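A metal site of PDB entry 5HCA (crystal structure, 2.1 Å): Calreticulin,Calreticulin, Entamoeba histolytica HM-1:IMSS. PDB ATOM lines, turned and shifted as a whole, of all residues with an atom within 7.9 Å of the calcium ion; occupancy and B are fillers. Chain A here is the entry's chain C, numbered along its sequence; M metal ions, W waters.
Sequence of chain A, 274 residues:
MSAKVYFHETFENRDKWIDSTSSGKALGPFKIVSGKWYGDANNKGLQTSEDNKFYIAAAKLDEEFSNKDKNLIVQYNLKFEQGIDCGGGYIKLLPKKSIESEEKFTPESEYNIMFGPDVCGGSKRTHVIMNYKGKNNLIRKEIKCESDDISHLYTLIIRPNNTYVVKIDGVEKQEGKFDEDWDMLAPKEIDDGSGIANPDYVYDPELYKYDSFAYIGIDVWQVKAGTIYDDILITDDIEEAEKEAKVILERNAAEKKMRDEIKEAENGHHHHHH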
ATOM      1  N   HIS A   8      24.185 -20.248  11.076  1.00  0.00           N
ATOM      2  CA  HIS A   8      22.802 -20.633  10.846  1.00  0.00           C
ATOM      3  C   HIS A   8      22.801 -22.117  10.530  1.00  0.00           C
ATOM      4  O   HIS A   8      23.103 -22.520   9.413  1.00  0.00           O
ATOM      5  CB  HIS A   8      22.133 -19.828   9.745  1.00  0.00           C
ATOM      6  CG  HIS A   8      20.694 -20.192   9.557  1.00  0.00           C
ATOM      7  ND1 HIS A   8      19.971 -19.861   8.434  1.00  0.00           N
ATOM      8  CD2 HIS A   8      19.858 -20.905  10.354  1.00  0.00           C
ATOM      9  CE1 HIS A   8      18.744 -20.345   8.551  1.00  0.00           C
ATOM     10  NE2 HIS A   8      18.651 -20.979   9.712  1.00  0.00           N
ATOM     11  N   GLU A   9      22.440 -22.905  11.530  1.00  0.00           N
ATOM     12  CA  GLU A   9      22.391 -24.345  11.456  1.00  0.00           C
ATOM     13  C   GLU A   9      20.940 -24.765  11.223  1.00  0.00           C
ATOM     14  O   GLU A   9      20.068 -24.484  12.059  1.00  0.00           O
ATOM     15  CB  GLU A   9      22.943 -24.950  12.749  1.00  0.00           C
ATOM     16  CG  GLU A   9      22.911 -26.457  12.815  1.00  0.00           C
ATOM     17  CD  GLU A   9      23.855 -27.099  11.797  1.00  0.00           C
ATOM     18  OE1 GLU A   9      25.085 -27.181  12.060  1.00  0.00           O
ATOM     19  OE2 GLU A   9      23.355 -27.493  10.725  1.00  0.00           O
ATOM     20  N   THR A  10      20.671 -25.410  10.097  1.00  0.00           N
ATOM     21  CA  THR A  10      19.365 -25.999   9.839  1.00  0.00           C
ATOM     22  C   THR A  10      19.346 -27.493  10.070  1.00  0.00           C
ATOM     23  O   THR A  10      18.281 -28.111   9.967  1.00  0.00           O
ATOM     24  CB  THR A  10      18.904 -25.688   8.403  1.00  0.00           C
ATOM     25  OG1 THR A  10      19.784 -26.303   7.470  1.00  0.00           O
ATOM     26  CG2 THR A  10      18.909 -24.190   8.146  1.00  0.00           C
ATOM     27  N   PHE A  11      20.503 -28.097  10.357  1.00  0.00           N
ATOM     28  CA  PHE A  11      20.640 -29.527  10.644  1.00  0.00           C
ATOM     29  C   PHE A  11      20.145 -30.413   9.500  1.00  0.00           C
ATOM     30  O   PHE A  11      19.451 -31.401   9.721  1.00  0.00           O
ATOM     31  CB  PHE A  11      19.939 -29.893  11.951  1.00  0.00           C
ATOM     32  CG  PHE A  11      20.702 -29.517  13.190  1.00  0.00           C
ATOM     33  CD1 PHE A  11      21.994 -30.011  13.417  1.00  0.00           C
ATOM     34  CD2 PHE A  11      20.125 -28.669  14.132  1.00  0.00           C
ATOM     35  CE1 PHE A  11      22.710 -29.669  14.561  1.00  0.00           C
ATOM     36  CE2 PHE A  11      20.825 -28.329  15.291  1.00  0.00           C
ATOM     37  CZ  PHE A  11      22.127 -28.832  15.508  1.00  0.00           C
ATOM     38  N   GLU A  12      20.494 -30.036   8.258  1.00  0.00           N
ATOM     39  CA  GLU A  12      20.460 -31.024   7.181  1.00  0.00           C
ATOM     40  C   GLU A  12      21.375 -32.205   7.500  1.00  0.00           C
ATOM     41  O   GLU A  12      21.083 -33.338   7.106  1.00  0.00           O
ATOM     42  CB  GLU A  12      20.885 -30.403   5.848  1.00  0.00           C
ATOM     43  CG  GLU A  12      19.979 -29.315   5.323  1.00  0.00           C
ATOM     44  CD  GLU A  12      20.428 -28.813   3.959  1.00  0.00           C
ATOM     45  OE1 GLU A  12      21.271 -29.501   3.345  1.00  0.00           O
ATOM     46  OE2 GLU A  12      19.937 -27.749   3.510  1.00  0.00           O
ATOM     47  N   VAL A  33      16.711 -36.252  12.373  1.00  0.00           N
ATOM     48  CA  VAL A  33      15.375 -36.832  12.217  1.00  0.00           C
ATOM     49  C   VAL A  33      14.351 -35.781  11.805  1.00  0.00           C
ATOM     50  O   VAL A  33      14.567 -34.577  11.938  1.00  0.00           O
ATOM     51  CB  VAL A  33      14.893 -37.534  13.515  1.00  0.00           C
ATOM     52  CG1 VAL A  33      15.943 -38.528  14.011  1.00  0.00           C
ATOM     53  CG2 VAL A  33      14.570 -36.503  14.587  1.00  0.00           C
ATOM     54  N   ASN A  42      10.684 -31.571   4.291  1.00  0.00           N
ATOM     55  CA  ASN A  42      12.099 -31.547   3.933  1.00  0.00           C
ATOM     56  C   ASN A  42      12.996 -31.014   5.061  1.00  0.00           C
ATOM     57  O   ASN A  42      14.223 -31.055   4.925  1.00  0.00           O
ATOM     58  CB  ASN A  42      12.320 -30.705   2.677  1.00  0.00           C
ATOM     59  CG  ASN A  42      11.650 -31.290   1.435  1.00  0.00           C
ATOM     60  OD1 ASN A  42      11.593 -32.510   1.254  1.00  0.00           O
ATOM     61  ND2 ASN A  42      11.147 -30.410   0.564  1.00  0.00           N
ATOM     62  N   ASN A  43      12.415 -30.526   6.150  1.00  0.00           N
ATOM     63  CA  ASN A  43      13.173 -30.008   7.278  1.00  0.00           C
ATOM     64  C   ASN A  43      13.512 -31.154   8.246  1.00  0.00           C
ATOM     65  O   ASN A  43      12.764 -32.121   8.354  1.00  0.00           O
ATOM     66  CB  ASN A  43      12.358 -28.933   7.974  1.00  0.00           C
ATOM     67  CG  ASN A  43      13.063 -28.346   9.162  1.00  0.00           C
ATOM     68  OD1 ASN A  43      14.235 -28.001   9.090  1.00  0.00           O
ATOM     69  ND2 ASN A  43      12.346 -28.236  10.276  1.00  0.00           N
ATOM     70  N   LYS A  44      14.653 -31.025   8.938  1.00  0.00           N
ATOM     71  CA  LYS A  44      15.070 -32.022   9.928  1.00  0.00           C
ATOM     72  C   LYS A  44      15.685 -31.342  11.148  1.00  0.00           C
ATOM     73  O   LYS A  44      15.944 -30.135  11.142  1.00  0.00           O
ATOM     74  CB  LYS A  44      16.080 -33.027   9.325  1.00  0.00           C
ATOM     75  CG  LYS A  44      15.544 -33.773   8.124  1.00  0.00           C
ATOM     76  CD  LYS A  44      16.252 -35.086   7.911  1.00  0.00           C
ATOM     77  CE  LYS A  44      15.705 -35.843   6.690  1.00  0.00           C
ATOM     78  NZ  LYS A  44      14.330 -36.363   6.910  1.00  0.00           N
ATOM     79  N   GLY A  45      15.950 -32.131  12.208  1.00  0.00           N
ATOM     80  CA  GLY A  45      16.483 -31.591  13.440  1.00  0.00           C
ATOM     81  C   GLY A  45      17.447 -32.559  14.115  1.00  0.00           C
ATOM     82  O   GLY A  45      17.559 -33.719  13.736  1.00  0.00           O
ATOM     83  N   LEU A  46      18.133 -32.055  15.145  1.00  0.00           N
ATOM     84  CA  LEU A  46      19.106 -32.853  15.892  1.00  0.00           C
ATOM     85  C   LEU A  46      18.465 -33.416  17.166  1.00  0.00           C
ATOM     86  O   LEU A  46      18.058 -32.648  18.043  1.00  0.00           O
ATOM     87  CB  LEU A  46      20.343 -32.012  16.220  1.00  0.00           C
ATOM     88  CG  LEU A  46      21.545 -32.753  16.834  1.00  0.00           C
ATOM     89  CD1 LEU A  46      22.430 -33.383  15.753  1.00  0.00           C
ATOM     90  CD2 LEU A  46      22.374 -31.848  17.760  1.00  0.00           C
ATOM     91  N   ASN A  77      15.107 -22.960  17.887  1.00  0.00           N
ATOM     92  CA  ASN A  77      13.823 -23.642  17.951  1.00  0.00           C
ATOM     93  C   ASN A  77      14.067 -25.014  18.598  1.00  0.00           C
ATOM     94  O   ASN A  77      14.893 -25.785  18.106  1.00  0.00           O
ATOM     95  CB  ASN A  77      13.260 -23.787  16.539  1.00  0.00           C
ATOM     96  CG  ASN A  77      11.756 -23.926  16.503  1.00  0.00           C
ATOM     97  OD1 ASN A  77      11.038 -23.301  17.275  1.00  0.00           O
ATOM     98  ND2 ASN A  77      11.279 -24.754  15.574  1.00  0.00           N
ATOM     99  N   ILE A 228      14.649 -32.355  20.490  1.00  0.00           N
ATOM    100  CA  ILE A 228      15.081 -32.000  19.138  1.00  0.00           C
ATOM    101  C   ILE A 228      15.480 -30.530  19.081  1.00  0.00           C
ATOM    102  O   ILE A 228      14.662 -29.637  19.371  1.00  0.00           O
ATOM    103  CB  ILE A 228      14.008 -32.305  18.078  1.00  0.00           C
ATOM    104  CG1 ILE A 228      13.764 -33.803  17.936  1.00  0.00           C
ATOM    105  CG2 ILE A 228      14.435 -31.725  16.709  1.00  0.00           C
ATOM    106  CD1 ILE A 228      12.500 -34.137  17.176  1.00  0.00           C
ATOM    107  N   TYR A 229      16.718 -30.275  18.657  1.00  0.00           N
ATOM    108  CA  TYR A 229      17.189 -28.945  18.279  1.00  0.00           C
ATOM    109  C   TYR A 229      16.926 -28.749  16.788  1.00  0.00           C
ATOM    110  O   TYR A 229      17.579 -29.380  15.946  1.00  0.00           O
ATOM    111  CB  TYR A 229      18.674 -28.796  18.613  1.00  0.00           C
ATOM    112  CG  TYR A 229      19.034 -28.838  20.101  1.00  0.00           C
ATOM    113  CD1 TYR A 229      19.101 -30.051  20.792  1.00  0.00           C
ATOM    114  CD2 TYR A 229      19.345 -27.683  20.788  1.00  0.00           C
ATOM    115  CE1 TYR A 229      19.453 -30.109  22.138  1.00  0.00           C
ATOM    116  CE2 TYR A 229      19.698 -27.716  22.132  1.00  0.00           C
ATOM    117  CZ  TYR A 229      19.757 -28.937  22.795  1.00  0.00           C
ATOM    118  OH  TYR A 229      20.110 -28.976  24.126  1.00  0.00           O
ATOM    119  N   ASP A 230      15.982 -27.868  16.448  1.00  0.00           N
ATOM    120  CA  ASP A 230      15.536 -27.764  15.061  1.00  0.00           C
ATOM    121  C   ASP A 230      16.375 -26.782  14.243  1.00  0.00           C
ATOM    122  O   ASP A 230      16.697 -27.055  13.077  1.00  0.00           O
ATOM    123  CB  ASP A 230      14.051 -27.352  15.048  1.00  0.00           C
ATOM    124  CG  ASP A 230      13.532 -27.053  13.655  1.00  0.00           C
ATOM    125  OD1 ASP A 230      13.838 -27.807  12.712  1.00  0.00           O
ATOM    126  OD2 ASP A 230      12.790 -26.056  13.505  1.00  0.00           O
ATOM    127  N   ASP A 231      16.752 -25.647  14.803  1.00  0.00           N
ATOM    128  CA  ASP A 231      17.314 -24.577  14.003  1.00  0.00           C
ATOM    129  C   ASP A 231      18.003 -23.613  14.966  1.00  0.00           C
ATOM    130  O   ASP A 231      17.471 -23.339  16.045  1.00  0.00           O
ATOM    131  CB  ASP A 231      16.225 -23.867  13.175  1.00  0.00           C
ATOM    132  CG  ASP A 231      16.780 -22.818  12.221  1.00  0.00           C
ATOM    133  OD1 ASP A 231      17.134 -21.693  12.668  1.00  0.00           O
ATOM    134  OD2 ASP A 231      16.844 -23.102  11.001  1.00  0.00           O
ATOM    135  N   ILE A 232      19.180 -23.131  14.584  1.00  0.00           N
ATOM    136  CA  ILE A 232      19.987 -22.260  15.446  1.00  0.00           C
ATOM    137  C   ILE A 232      20.484 -21.092  14.622  1.00  0.00           C
ATOM    138  O   ILE A 232      21.116 -21.289  13.582  1.00  0.00           O
ATOM    139  CB  ILE A 232      21.167 -23.009  16.094  1.00  0.00           C
ATOM    140  CG1 ILE A 232      20.675 -24.243  16.831  1.00  0.00           C
ATOM    141  CG2 ILE A 232      21.891 -22.093  17.064  1.00  0.00           C
ATOM    142  CD1 ILE A 232      21.787 -25.083  17.424  1.00  0.00           C
ATOM    143  N   ILE A 248      10.045 -19.527  10.755  1.00  0.00           N
ATOM    144  CA  ILE A 248       9.980 -20.595  11.748  1.00  0.00           C
ATOM    145  C   ILE A 248       8.628 -20.615  12.465  1.00  0.00           C
ATOM    146  O   ILE A 248       8.047 -21.680  12.679  1.00  0.00           O
ATOM    147  CB  ILE A 248      11.143 -20.458  12.740  1.00  0.00           C
ATOM    148  CG1 ILE A 248      12.431 -20.958  12.061  1.00  0.00           C
ATOM    149  CG2 ILE A 248      10.843 -21.253  13.995  1.00  0.00           C
ATOM    150  CD1 ILE A 248      13.705 -20.620  12.782  1.00  0.00           C
ATOM    151  N   ARG A 251       6.125 -22.216  10.341  1.00  0.00           N
ATOM    152  CA  ARG A 251       6.312 -23.659  10.241  1.00  0.00           C
ATOM    153  C   ARG A 251       5.918 -24.363  11.536  1.00  0.00           C
ATOM    154  O   ARG A 251       5.405 -25.486  11.500  1.00  0.00           O
ATOM    155  CB  ARG A 251       7.761 -23.982   9.847  1.00  0.00           C
ATOM    156  CG  ARG A 251       8.040 -25.455   9.725  1.00  0.00           C
ATOM    157  CD  ARG A 251       9.436 -25.683   9.153  1.00  0.00           C
ATOM    158  NE  ARG A 251      10.490 -25.347  10.106  1.00  0.00           N
ATOM    159  CZ  ARG A 251      11.769 -25.188   9.765  1.00  0.00           C
ATOM    160  NH1 ARG A 251      12.124 -25.325   8.500  1.00  0.00           N
ATOM    161  NH2 ARG A 251      12.678 -24.906  10.681  1.00  0.00           N
HETATM  162 CA    CA M   1      15.912 -27.787  10.964  1.00  0.00          CA
HETATM  163  O   HOH W   1      15.883 -25.259  10.123  1.00  0.00           O
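Water W1 lies within hydrogen-bond range of the side-chain carboxylate of Asp 231 and the guanidinium group of Arg 251.
The calcium ion is bound by the backbone carbonyl oxygen (O) of Lys 44 (2.4 Å), the backbone carbonyl oxygen (O) of Asp 230 (2.4 Å), the side-chain amide oxygen (OD1) of Asn 43 (2.5 Å), the backbone carbonyl oxygen (O) of Thr 10 (2.6 Å), water W1 (2.7 Å) and the side-chain carboxylate (OD1) of Asp 230 (2.7 Å).
The side-chain amide nitrogen (ND2) of Asn 43 sits close to the guanidinium group (NH2) of Arg 251.
OD2 of Asp 230 lies within hydrogen-bond range of ND2 of Asn 77, 2.9 Å away.
OD2 of Asp 230 is in salt-bridge range of NH2 of Arg 251 (3.1 Å).
Along chain A the residues within 4 Å of the calcium ion span positions 10 to 230.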
